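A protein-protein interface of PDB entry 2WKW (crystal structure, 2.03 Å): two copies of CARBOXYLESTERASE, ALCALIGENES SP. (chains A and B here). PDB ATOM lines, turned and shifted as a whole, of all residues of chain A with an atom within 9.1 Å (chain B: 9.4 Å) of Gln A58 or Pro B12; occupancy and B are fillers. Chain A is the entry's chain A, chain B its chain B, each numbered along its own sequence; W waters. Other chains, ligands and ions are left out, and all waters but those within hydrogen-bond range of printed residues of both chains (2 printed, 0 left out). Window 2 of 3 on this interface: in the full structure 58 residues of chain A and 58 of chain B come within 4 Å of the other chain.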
ATOM      1  N   PRO A  12      -9.888 -28.265 -16.604  1.00  0.00           N
ATOM      2  CA  PRO A  12     -10.636 -27.132 -16.074  1.00  0.00           C
ATOM      3  C   PRO A  12      -9.825 -26.274 -15.115  1.00  0.00           C
ATOM      4  O   PRO A  12      -8.756 -26.680 -14.666  1.00  0.00           O
ATOM      5  CB  PRO A  12     -11.798 -27.797 -15.334  1.00  0.00           C
ATOM      6  CG  PRO A  12     -11.278 -29.141 -14.950  1.00  0.00           C
ATOM      7  CD  PRO A  12     -10.385 -29.552 -16.077  1.00  0.00           C
ATOM      8  N   LEU A  13     -10.333 -25.084 -14.822  1.00  0.00           N
ATOM      9  CA  LEU A  13      -9.699 -24.206 -13.864  1.00  0.00           C
ATOM     10  C   LEU A  13     -10.710 -23.774 -12.819  1.00  0.00           C
ATOM     11  O   LEU A  13     -11.809 -23.339 -13.153  1.00  0.00           O
ATOM     12  CB  LEU A  13      -9.091 -22.999 -14.572  1.00  0.00           C
ATOM     13  CG  LEU A  13      -8.614 -21.839 -13.689  1.00  0.00           C
ATOM     14  CD1 LEU A  13      -7.367 -22.203 -12.872  1.00  0.00           C
ATOM     15  CD2 LEU A  13      -8.374 -20.633 -14.564  1.00  0.00           C
ATOM     16  N   THR A  14     -10.328 -23.888 -11.552  1.00  0.00           N
ATOM     17  CA  THR A  14     -11.218 -23.541 -10.465  1.00  0.00           C
ATOM     18  C   THR A  14     -10.754 -22.250  -9.829  1.00  0.00           C
ATOM     19  O   THR A  14      -9.566 -22.061  -9.570  1.00  0.00           O
ATOM     20  CB  THR A  14     -11.348 -24.677  -9.423  1.00  0.00           C
ATOM     21  OG1 THR A  14     -11.937 -25.811 -10.064  1.00  0.00           O
ATOM     22  CG2 THR A  14     -12.289 -24.264  -8.299  1.00  0.00           C
ATOM     23  N   LEU A  15     -11.706 -21.350  -9.635  1.00  0.00           N
ATOM     24  CA  LEU A  15     -11.438 -20.048  -9.066  1.00  0.00           C
ATOM     25  C   LEU A  15     -12.081 -19.960  -7.708  1.00  0.00           C
ATOM     26  O   LEU A  15     -13.280 -20.213  -7.566  1.00  0.00           O
ATOM     27  CB  LEU A  15     -12.021 -18.960  -9.967  1.00  0.00           C
ATOM     28  CG  LEU A  15     -11.331 -18.878 -11.333  1.00  0.00           C
ATOM     29  CD1 LEU A  15     -11.751 -17.632 -12.064  1.00  0.00           C
ATOM     30  CD2 LEU A  15      -9.828 -18.884 -11.130  1.00  0.00           C
ATOM     31  N   SER A  16     -11.289 -19.587  -6.720  1.00  0.00           N
ATOM     32  CA  SER A  16     -11.837 -19.255  -5.423  1.00  0.00           C
ATOM     33  C   SER A  16     -12.691 -17.980  -5.524  1.00  0.00           C
ATOM     34  O   SER A  16     -13.716 -17.847  -4.846  1.00  0.00           O
ATOM     35  CB  SER A  16     -10.696 -19.113  -4.417  1.00  0.00           C
ATOM     36  OG  SER A  16     -11.127 -18.487  -3.237  1.00  0.00           O
ATOM     37  N   GLY A  17     -12.286 -17.042  -6.378  1.00  0.00           N
ATOM     38  CA  GLY A  17     -13.086 -15.830  -6.591  1.00  0.00           C
ATOM     39  C   GLY A  17     -12.754 -15.082  -7.877  1.00  0.00           C
ATOM     40  O   GLY A  17     -11.682 -15.290  -8.476  1.00  0.00           O
ATOM     41  N   GLN A  18     -13.692 -14.243  -8.317  1.00  0.00           N
ATOM     42  CA  GLN A  18     -13.455 -13.319  -9.439  1.00  0.00           C
ATOM     43  C   GLN A  18     -14.275 -12.035  -9.305  1.00  0.00           C
ATOM     44  O   GLN A  18     -15.336 -12.025  -8.676  1.00  0.00           O
ATOM     45  CB  GLN A  18     -13.696 -13.993 -10.799  1.00  0.00           C
ATOM     46  CG  GLN A  18     -15.133 -14.439 -11.116  1.00  0.00           C
ATOM     47  CD  GLN A  18     -15.318 -14.805 -12.611  1.00  0.00           C
ATOM     48  OE1 GLN A  18     -16.398 -14.615 -13.187  1.00  0.00           O
ATOM     49  NE2 GLN A  18     -14.248 -15.287 -13.247  1.00  0.00           N
ATOM     50  N   GLN A  55      -8.826 -12.366 -10.754  1.00  0.00           N
ATOM     51  CA  GLN A  55      -9.179 -13.761 -10.562  1.00  0.00           C
ATOM     52  C   GLN A  55      -8.278 -14.363  -9.495  1.00  0.00           C
ATOM     53  O   GLN A  55      -7.077 -14.085  -9.450  1.00  0.00           O
ATOM     54  CB  GLN A  55      -9.123 -14.528 -11.881  1.00  0.00           C
ATOM     55  CG  GLN A  55     -10.239 -14.075 -12.814  1.00  0.00           C
ATOM     56  CD  GLN A  55     -10.299 -14.844 -14.116  1.00  0.00           C
ATOM     57  OE1 GLN A  55     -11.317 -15.455 -14.450  1.00  0.00           O
ATOM     58  NE2 GLN A  55      -9.215 -14.823 -14.846  1.00  0.00           N
ATOM     59  N   ILE A  56      -8.887 -15.161  -8.621  1.00  0.00           N
ATOM     60  CA  ILE A  56      -8.194 -15.727  -7.460  1.00  0.00           C
ATOM     61  C   ILE A  56      -8.263 -17.250  -7.545  1.00  0.00           C
ATOM     62  O   ILE A  56      -9.352 -17.822  -7.509  1.00  0.00           O
ATOM     63  CB  ILE A  56      -8.833 -15.224  -6.139  1.00  0.00           C
ATOM     64  CG1 ILE A  56      -8.766 -13.691  -6.055  1.00  0.00           C
ATOM     65  CG2 ILE A  56      -8.157 -15.835  -4.918  1.00  0.00           C
ATOM     66  CD1 ILE A  56      -9.288 -13.118  -4.746  1.00  0.00           C
ATOM     67  N   PRO A  57      -7.091 -17.919  -7.684  1.00  0.00           N
ATOM     68  CA  PRO A  57      -7.123 -19.390  -7.730  1.00  0.00           C
ATOM     69  C   PRO A  57      -7.310 -19.949  -6.313  1.00  0.00           C
ATOM     70  O   PRO A  57      -7.197 -19.195  -5.342  1.00  0.00           O
ATOM     71  CB  PRO A  57      -5.720 -19.749  -8.240  1.00  0.00           C
ATOM     72  CG  PRO A  57      -4.835 -18.641  -7.654  1.00  0.00           C
ATOM     73  CD  PRO A  57      -5.704 -17.398  -7.702  1.00  0.00           C
ATOM     74  N   GLN A  58      -7.585 -21.246  -6.188  1.00  0.00           N
ATOM     75  CA  GLN A  58      -7.619 -21.874  -4.857  1.00  0.00           C
ATOM     76  C   GLN A  58      -6.220 -21.907  -4.289  1.00  0.00           C
ATOM     77  O   GLN A  58      -5.236 -21.999  -5.048  1.00  0.00           O
ATOM     78  CB  GLN A  58      -8.200 -23.288  -4.906  1.00  0.00           C
ATOM     79  CG  GLN A  58      -9.594 -23.339  -5.484  1.00  0.00           C
ATOM     80  CD  GLN A  58     -10.200 -24.724  -5.407  1.00  0.00           C
ATOM     81  OE1 GLN A  58      -9.755 -25.650  -6.088  1.00  0.00           O
ATOM     82  NE2 GLN A  58     -11.232 -24.872  -4.582  1.00  0.00           N
ATOM     83  N   ARG A  59      -6.127 -21.785  -2.963  1.00  0.00           N
ATOM     84  CA  ARG A  59      -4.858 -21.815  -2.246  1.00  0.00           C
ATOM     85  C   ARG A  59      -3.859 -20.850  -2.907  1.00  0.00           C
ATOM     86  O   ARG A  59      -2.687 -21.168  -3.149  1.00  0.00           O
ATOM     87  CB  ARG A  59      -4.351 -23.261  -2.128  1.00  0.00           C
ATOM     88  CG  ARG A  59      -5.266 -24.148  -1.250  1.00  0.00           C
ATOM     89  CD  ARG A  59      -5.094 -25.654  -1.510  1.00  0.00           C
ATOM     90  NE  ARG A  59      -5.890 -26.136  -2.642  1.00  0.00           N
ATOM     91  CZ  ARG A  59      -7.144 -26.580  -2.552  1.00  0.00           C
ATOM     92  NH1 ARG A  59      -7.770 -26.606  -1.383  1.00  0.00           N
ATOM     93  NH2 ARG A  59      -7.780 -26.993  -3.640  1.00  0.00           N
ATOM     94  N   ALA A  60      -4.348 -19.639  -3.171  1.00  0.00           N
ATOM     95  CA  ALA A  60      -3.577 -18.603  -3.864  1.00  0.00           C
ATOM     96  C   ALA A  60      -2.267 -18.303  -3.150  1.00  0.00           C
ATOM     97  O   ALA A  60      -2.223 -18.305  -1.915  1.00  0.00           O
ATOM     98  CB  ALA A  60      -4.420 -17.332  -3.988  1.00  0.00           C
ATOM     99  N   LYS A  61      -1.202 -18.051  -3.913  1.00  0.00           N
ATOM    100  CA  LYS A  61       0.066 -17.611  -3.321  1.00  0.00           C
ATOM    101  C   LYS A  61      -0.096 -16.246  -2.638  1.00  0.00           C
ATOM    102  O   LYS A  61      -1.051 -15.522  -2.917  1.00  0.00           O
ATOM    103  CB  LYS A  61       1.190 -17.583  -4.358  1.00  0.00           C
ATOM    104  CG  LYS A  61       1.565 -18.976  -4.852  1.00  0.00           C
ATOM    105  CD  LYS A  61       2.533 -18.909  -6.003  1.00  0.00           C
ATOM    106  CE  LYS A  61       2.850 -20.289  -6.552  1.00  0.00           C
ATOM    107  NZ  LYS A  61       3.645 -21.081  -5.566  1.00  0.00           N
ATOM    108  N   PHE A  92      -0.820 -17.761 -15.185  1.00  0.00           N
ATOM    109  CA  PHE A  92      -0.457 -17.374 -13.816  1.00  0.00           C
ATOM    110  C   PHE A  92      -1.455 -17.939 -12.808  1.00  0.00           C
ATOM    111  O   PHE A  92      -1.066 -18.432 -11.744  1.00  0.00           O
ATOM    112  CB  PHE A  92      -0.375 -15.845 -13.667  1.00  0.00           C
ATOM    113  CG  PHE A  92       0.797 -15.217 -14.365  1.00  0.00           C
ATOM    114  CD1 PHE A  92       1.783 -15.993 -14.968  1.00  0.00           C
ATOM    115  CD2 PHE A  92       0.944 -13.827 -14.372  1.00  0.00           C
ATOM    116  CE1 PHE A  92       2.889 -15.385 -15.604  1.00  0.00           C
ATOM    117  CE2 PHE A  92       2.042 -13.212 -14.993  1.00  0.00           C
ATOM    118  CZ  PHE A  92       3.012 -13.987 -15.612  1.00  0.00           C
ATOM    119  N   LEU A  93      -2.739 -17.841 -13.158  1.00  0.00           N
ATOM    120  CA  LEU A  93      -3.822 -18.407 -12.345  1.00  0.00           C
ATOM    121  C   LEU A  93      -3.615 -19.910 -12.109  1.00  0.00           C
ATOM    122  O   LEU A  93      -3.674 -20.374 -10.967  1.00  0.00           O
ATOM    123  CB  LEU A  93      -5.177 -18.174 -13.015  1.00  0.00           C
ATOM    124  CG  LEU A  93      -5.645 -16.729 -13.105  1.00  0.00           C
ATOM    125  CD1 LEU A  93      -6.836 -16.631 -14.029  1.00  0.00           C
ATOM    126  CD2 LEU A  93      -5.953 -16.182 -11.712  1.00  0.00           C
ATOM    127  N   ARG A  94      -3.367 -20.658 -13.180  1.00  0.00           N
ATOM    128  CA  ARG A  94      -3.085 -22.098 -13.094  1.00  0.00           C
ATOM    129  C   ARG A  94      -1.829 -22.417 -12.279  1.00  0.00           C
ATOM    130  O   ARG A  94      -1.734 -23.504 -11.722  1.00  0.00           O
ATOM    131  CB  ARG A  94      -2.998 -22.723 -14.485  1.00  0.00           C
ATOM    132  CG  ARG A  94      -4.332 -22.712 -15.225  1.00  0.00           C
ATOM    133  CD  ARG A  94      -4.204 -23.275 -16.632  1.00  0.00           C
ATOM    134  NE  ARG A  94      -5.516 -23.350 -17.291  1.00  0.00           N
ATOM    135  CZ  ARG A  94      -6.406 -24.325 -17.100  1.00  0.00           C
ATOM    136  NH1 ARG A  94      -6.136 -25.340 -16.274  1.00  0.00           N
ATOM    137  NH2 ARG A  94      -7.569 -24.294 -17.738  1.00  0.00           N
ATOM    138  N   LYS A  95      -0.893 -21.470 -12.173  1.00  0.00           N
ATOM    139  CA  LYS A  95       0.321 -21.667 -11.373  1.00  0.00           C
ATOM    140  C   LYS A  95       0.127 -21.206  -9.931  1.00  0.00           C
ATOM    141  O   LYS A  95       1.092 -21.136  -9.167  1.00  0.00           O
ATOM    142  CB  LYS A  95       1.523 -20.915 -11.975  1.00  0.00           C
ATOM    143  CG  LYS A  95       1.916 -21.321 -13.405  1.00  0.00           C
ATOM    144  CD  LYS A  95       2.046 -22.838 -13.585  1.00  0.00           C
ATOM    145  CE  LYS A  95       3.393 -23.349 -13.136  1.00  0.00           C
ATOM    146  NZ  LYS A  95       3.458 -24.829 -13.294  1.00  0.00           N
ATOM    147  N   GLY A  96      -1.106 -20.853  -9.574  1.00  0.00           N
ATOM    148  CA  GLY A  96      -1.411 -20.495  -8.192  1.00  0.00           C
ATOM    149  C   GLY A  96      -1.309 -19.017  -7.830  1.00  0.00           C
ATOM    150  O   GLY A  96      -1.389 -18.680  -6.651  1.00  0.00           O
ATOM    151  N   TYR A  97      -1.148 -18.129  -8.822  1.00  0.00           N
ATOM    152  CA  TYR A  97      -1.101 -16.678  -8.548  1.00  0.00           C
ATOM    153  C   TYR A  97      -2.441 -16.002  -8.808  1.00  0.00           C
ATOM    154  O   TYR A  97      -3.053 -16.191  -9.872  1.00  0.00           O
ATOM    155  CB  TYR A  97      -0.039 -15.972  -9.407  1.00  0.00           C
ATOM    156  CG  TYR A  97       1.391 -16.330  -9.074  1.00  0.00           C
ATOM    157  CD1 TYR A  97       2.114 -15.584  -8.139  1.00  0.00           C
ATOM    158  CD2 TYR A  97       2.014 -17.432  -9.666  1.00  0.00           C
ATOM    159  CE1 TYR A  97       3.428 -15.909  -7.815  1.00  0.00           C
ATOM    160  CE2 TYR A  97       3.333 -17.759  -9.356  1.00  0.00           C
ATOM    161  CZ  TYR A  97       4.029 -16.991  -8.426  1.00  0.00           C
ATOM    162  OH  TYR A  97       5.332 -17.306  -8.115  1.00  0.00           O
ATOM    163  N   SER A  98      -2.886 -15.201  -7.843  1.00  0.00           N
ATOM    164  CA  SER A  98      -3.986 -14.264  -8.077  1.00  0.00           C
ATOM    165  C   SER A  98      -3.507 -13.216  -9.091  1.00  0.00           C
ATOM    166  O   SER A  98      -2.357 -12.767  -9.037  1.00  0.00           O
ATOM    167  CB  SER A  98      -4.402 -13.578  -6.762  1.00  0.00           C
ATOM    168  OG  SER A  98      -4.982 -14.510  -5.849  1.00  0.00           O
ATOM    169  N   PRO B   9     -25.048 -18.117  -4.799  1.00  0.00           N
ATOM    170  CA  PRO B   9     -24.243 -19.343  -4.735  1.00  0.00           C
ATOM    171  C   PRO B   9     -22.780 -19.029  -4.382  1.00  0.00           C
ATOM    172  O   PRO B   9     -22.033 -18.526  -5.224  1.00  0.00           O
ATOM    173  CB  PRO B   9     -24.368 -19.923  -6.152  1.00  0.00           C
ATOM    174  CG  PRO B   9     -25.644 -19.389  -6.669  1.00  0.00           C
ATOM    175  CD  PRO B   9     -25.760 -18.002  -6.085  1.00  0.00           C
ATOM    176  N   ALA B  10     -22.397 -19.295  -3.132  1.00  0.00           N
ATOM    177  CA  ALA B  10     -21.029 -19.065  -2.664  1.00  0.00           C
ATOM    178  C   ALA B  10     -20.124 -20.258  -3.026  1.00  0.00           C
ATOM    179  O   ALA B  10     -20.576 -21.226  -3.658  1.00  0.00           O
ATOM    180  CB  ALA B  10     -21.017 -18.788  -1.149  1.00  0.00           C
ATOM    181  N   GLY B  11     -18.850 -20.181  -2.642  1.00  0.00           N
ATOM    182  CA  GLY B  11     -17.892 -21.243  -2.961  1.00  0.00           C
ATOM    183  C   GLY B  11     -17.232 -21.038  -4.314  1.00  0.00           C
ATOM    184  O   GLY B  11     -17.512 -20.044  -4.992  1.00  0.00           O
ATOM    185  N   PRO B  12     -16.336 -21.970  -4.713  1.00  0.00           N
ATOM    186  CA  PRO B  12     -15.533 -21.769  -5.917  1.00  0.00           C
ATOM    187  C   PRO B  12     -16.295 -22.004  -7.218  1.00  0.00           C
ATOM    188  O   PRO B  12     -17.362 -22.623  -7.227  1.00  0.00           O
ATOM    189  CB  PRO B  12     -14.404 -22.799  -5.765  1.00  0.00           C
ATOM    190  CG  PRO B  12     -15.002 -23.887  -4.941  1.00  0.00           C
ATOM    191  CD  PRO B  12     -15.909 -23.172  -3.966  1.00  0.00           C
ATOM    192  N   LEU B  13     -15.726 -21.505  -8.308  1.00  0.00           N
ATOM    193  CA  LEU B  13     -16.323 -21.626  -9.616  1.00  0.00           C
ATOM    194  C   LEU B  13     -15.339 -22.340 -10.531  1.00  0.00           C
ATOM    195  O   LEU B  13     -14.175 -21.945 -10.638  1.00  0.00           O
ATOM    196  CB  LEU B  13     -16.647 -20.237 -10.132  1.00  0.00           C
ATOM    197  CG  LEU B  13     -16.975 -19.991 -11.597  1.00  0.00           C
ATOM    198  CD1 LEU B  13     -18.200 -20.778 -12.039  1.00  0.00           C
ATOM    199  CD2 LEU B  13     -17.187 -18.497 -11.764  1.00  0.00           C
ATOM    200  N   THR B  14     -15.814 -23.386 -11.194  1.00  0.00           N
ATOM    201  CA  THR B  14     -14.971 -24.154 -12.091  1.00  0.00           C
ATOM    202  C   THR B  14     -15.315 -23.893 -13.550  1.00  0.00           C
ATOM    203  O   THR B  14     -16.477 -23.971 -13.962  1.00  0.00           O
ATOM    204  CB  THR B  14     -15.002 -25.656 -11.749  1.00  0.00           C
ATOM    205  OG1 THR B  14     -14.550 -25.818 -10.397  1.00  0.00           O
ATOM    206  CG2 THR B  14     -14.049 -26.448 -12.669  1.00  0.00           C
ATOM    207  N   LEU B  15     -14.278 -23.574 -14.319  1.00  0.00           N
ATOM    208  CA  LEU B  15     -14.426 -23.237 -15.721  1.00  0.00           C
ATOM    209  C   LEU B  15     -13.876 -24.359 -16.584  1.00  0.00           C
ATOM    210  O   LEU B  15     -12.709 -24.723 -16.475  1.00  0.00           O
ATOM    211  CB  LEU B  15     -13.660 -21.941 -16.026  1.00  0.00           C
ATOM    212  CG  LEU B  15     -14.085 -20.744 -15.155  1.00  0.00           C
ATOM    213  CD1 LEU B  15     -13.116 -19.581 -15.288  1.00  0.00           C
ATOM    214  CD2 LEU B  15     -15.484 -20.339 -15.542  1.00  0.00           C
ATOM    215  N   GLN B  58     -18.518 -26.170 -16.615  1.00  0.00           N
ATOM    216  CA  GLN B  58     -18.640 -27.616 -16.830  1.00  0.00           C
ATOM    217  C   GLN B  58     -20.088 -28.007 -17.143  1.00  0.00           C
ATOM    218  O   GLN B  58     -21.026 -27.408 -16.617  1.00  0.00           O
ATOM    219  CB  GLN B  58     -18.129 -28.372 -15.609  1.00  0.00           C
ATOM    220  CG  GLN B  58     -16.636 -28.204 -15.403  1.00  0.00           C
ATOM    221  CD  GLN B  58     -16.098 -29.028 -14.251  1.00  0.00           C
ATOM    222  OE1 GLN B  58     -15.149 -29.792 -14.414  1.00  0.00           O
ATOM    223  NE2 GLN B  58     -16.693 -28.870 -13.081  1.00  0.00           N
ATOM    224  N   MET B  86     -22.084 -10.200  -6.597  1.00  0.00           N
ATOM    225  CA  MET B  86     -22.022 -11.027  -7.787  1.00  0.00           C
ATOM    226  C   MET B  86     -22.859 -10.394  -8.884  1.00  0.00           C
ATOM    227  O   MET B  86     -23.985  -9.969  -8.625  1.00  0.00           O
ATOM    228  CB  MET B  86     -22.552 -12.432  -7.467  1.00  0.00           C
ATOM    229  CG  MET B  86     -22.429 -13.421  -8.622  1.00  0.00           C
ATOM    230  SD  MET B  86     -23.101 -15.061  -8.283  1.00  0.00           S
ATOM    231  CE  MET B  86     -22.166 -15.551  -6.843  1.00  0.00           C
ATOM    232  N   GLU B  90     -21.053 -13.814 -13.738  1.00  0.00           N
ATOM    233  CA  GLU B  90     -20.705 -14.884 -12.818  1.00  0.00           C
ATOM    234  C   GLU B  90     -21.912 -15.777 -12.484  1.00  0.00           C
ATOM    235  O   GLU B  90     -21.784 -17.008 -12.383  1.00  0.00           O
ATOM    236  CB  GLU B  90     -20.103 -14.314 -11.526  1.00  0.00           C
ATOM    237  CG  GLU B  90     -19.714 -15.428 -10.543  1.00  0.00           C
ATOM    238  CD  GLU B  90     -19.113 -14.922  -9.252  1.00  0.00           C
ATOM    239  OE1 GLU B  90     -18.730 -13.727  -9.166  1.00  0.00           O
ATOM    240  OE2 GLU B  90     -19.026 -15.742  -8.316  1.00  0.00           O
ATOM    241  N   LEU B  93     -22.906 -18.205 -15.321  1.00  0.00           N
ATOM    242  CA  LEU B  93     -21.897 -19.269 -15.292  1.00  0.00           C
ATOM    243  C   LEU B  93     -22.193 -20.319 -14.224  1.00  0.00           C
ATOM    244  O   LEU B  93     -22.132 -21.519 -14.494  1.00  0.00           O
ATOM    245  CB  LEU B  93     -20.495 -18.690 -15.066  1.00  0.00           C
ATOM    246  CG  LEU B  93     -19.959 -17.827 -16.206  1.00  0.00           C
ATOM    247  CD1 LEU B  93     -18.680 -17.124 -15.802  1.00  0.00           C
ATOM    248  CD2 LEU B  93     -19.765 -18.658 -17.465  1.00  0.00           C
ATOM    249  N   ARG B  94     -22.513 -19.865 -13.010  1.00  0.00           N
ATOM    250  CA  ARG B  94     -22.793 -20.770 -11.895  1.00  0.00           C
ATOM    251  C   ARG B  94     -24.069 -21.568 -12.149  1.00  0.00           C
ATOM    252  O   ARG B  94     -24.218 -22.676 -11.637  1.00  0.00           O
ATOM    253  CB  ARG B  94     -22.876 -20.015 -10.567  1.00  0.00           C
ATOM    254  CG  ARG B  94     -21.548 -19.442 -10.122  1.00  0.00           C
ATOM    255  CD  ARG B  94     -21.674 -18.772  -8.754  1.00  0.00           C
ATOM    256  NE  ARG B  94     -20.404 -18.240  -8.270  1.00  0.00           N
ATOM    257  CZ  ARG B  94     -19.517 -18.942  -7.565  1.00  0.00           C
ATOM    258  NH1 ARG B  94     -19.746 -20.223  -7.281  1.00  0.00           N
ATOM    259  NH2 ARG B  94     -18.386 -18.376  -7.153  1.00  0.00           N
HETATM  260  O   HOH W   1     -16.455 -16.639  -5.144  1.00  0.00           O
HETATM  261  O   HOH W   2     -14.696 -19.897  -3.077  1.00  0.00           O
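The backbone NH (N) of Leu B15 lies within hydrogen-bond range of the backbone carbonyl oxygen (O) of Leu A13, 2.7 Å away.
The side-chain hydroxyl of Thr A14 sits at hydrogen-bond distance from the side-chain hydroxyl of Thr B14 (2.6 Å).
The backbone NH (N) of Leu A15 is in hydrogen-bond range of the backbone carbonyl oxygen (O) of Leu B13 (2.7 Å).
Pro A12 touches Thr B14, and with the chains exchanged Thr A14 touches Pro B12.
Pro A12 touches Gln B58, and with the chains exchanged Gln A58 touches Pro B12.
Leu A13 touches Leu B15, and with the chains exchanged Leu A15 touches Leu B13.
Thr B14 touches its own counterpart, Thr A14.
7 positions are printed for both chains.
The backbone carbonyl oxygen (O) of Pro A12 is in hydrogen-bond range of the guanidinium group (NH1) of Arg A94 (3.4 Å).
NE2 of Gln A18 lies within hydrogen-bond range of OE1 of Gln A55, at 3.2 Å.
OE1 of Gln A58 lies within hydrogen-bond range of NH2 of Arg A59 (3.4 Å).
The backbone carbonyl oxygen (O) of Pro B12 is in hydrogen-bond range of the guanidinium group (NH1) of Arg B94, 3.4 Å away.
The side-chain carboxylate (OE2) of Glu B90 is in salt-bridge range of the guanidinium group (NE) of Arg B94 (2.9 Å).
Gln A58 touches just one residue of chain B: Pro B12 (3.9 Å).
Pro B12 touches just these residues of chain A: Thr A14, Leu A15 and Gln A58.
Printed residues of chain A within 4 Å of Leu B15: Pro A12 (3.2 Å) and Leu A13 (2.7 Å).
Printed residues of chain A within 4 Å of Thr B14: Pro A12 (3.7 Å), Leu A13 (3.4 Å) and Thr A14 (2.6 Å).
Of the printed residues of chain B, Pro A12 touches Thr B14 (3.7 Å), Leu B15 (3.2 Å) and Gln B58 (3.96 Å).
Of the printed residues of chain B, Leu A13 touches Leu B13 (3.7 Å), Thr B14 (3.4 Å) and Leu B15 (2.7 Å).
Of the printed residues of chain B, Leu A15 touches Pro B12 (3.2 Å) and Leu B13 (2.7 Å).
Gly A17 touches none of the printed residues of chain B.
Pro B9 touches none of the printed residues of chain A.
The nearest residue of chain B that does not touch Gln A58 is Thr B14 (6.4 Å).
The nearest printed residue of chain B that does not touch Pro A12 is Leu B13 (7.6 Å).
Water W2 bridges the backbone carbonyl oxygen of Ser A16 (2.9 Å) and the backbone carbonyl oxygen of Gly B11 (3.4 Å).
Water W1 bridges the backbone carbonyl oxygen of Ser A16 and the guanidinium group of Arg B94.
CG2 of Thr B14 touches CB of Pro A12 (3.7 Å).
Pro A12 touches Leu B15 (CA to O, 3.2 Å).
Gln B58 touches Pro A12.
Leu B13 touches Leu A13.
O of Leu A13 touches CA of Thr B14, at 3.4 Å.
Pro B12 touches Thr A14 (CB to CG2, 3.6 Å).
O of Leu B13 touches CA of Thr A14, at 3.4 Å.
O of Leu A15 touches CA of Pro B12, at 3.2 Å.
Gln A18 touches Glu B90.
Gln A58 touches Pro B12.
Printed residues of chain A that touch a printed residue of chain B: Pro A12, Leu A13, Thr A14, Leu A15, Gln A18 and Gln A58.
Hydrophobic or aromatic side chains of chain A that line the printed part of chain B: Pro A12 and Leu A15.
Of the 12 printed residues of chain B, 6 touch a printed residue of chain A.
Hydrophobic or aromatic side chains of chain B that line the printed part of chain A: Pro B12 and Leu B15.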
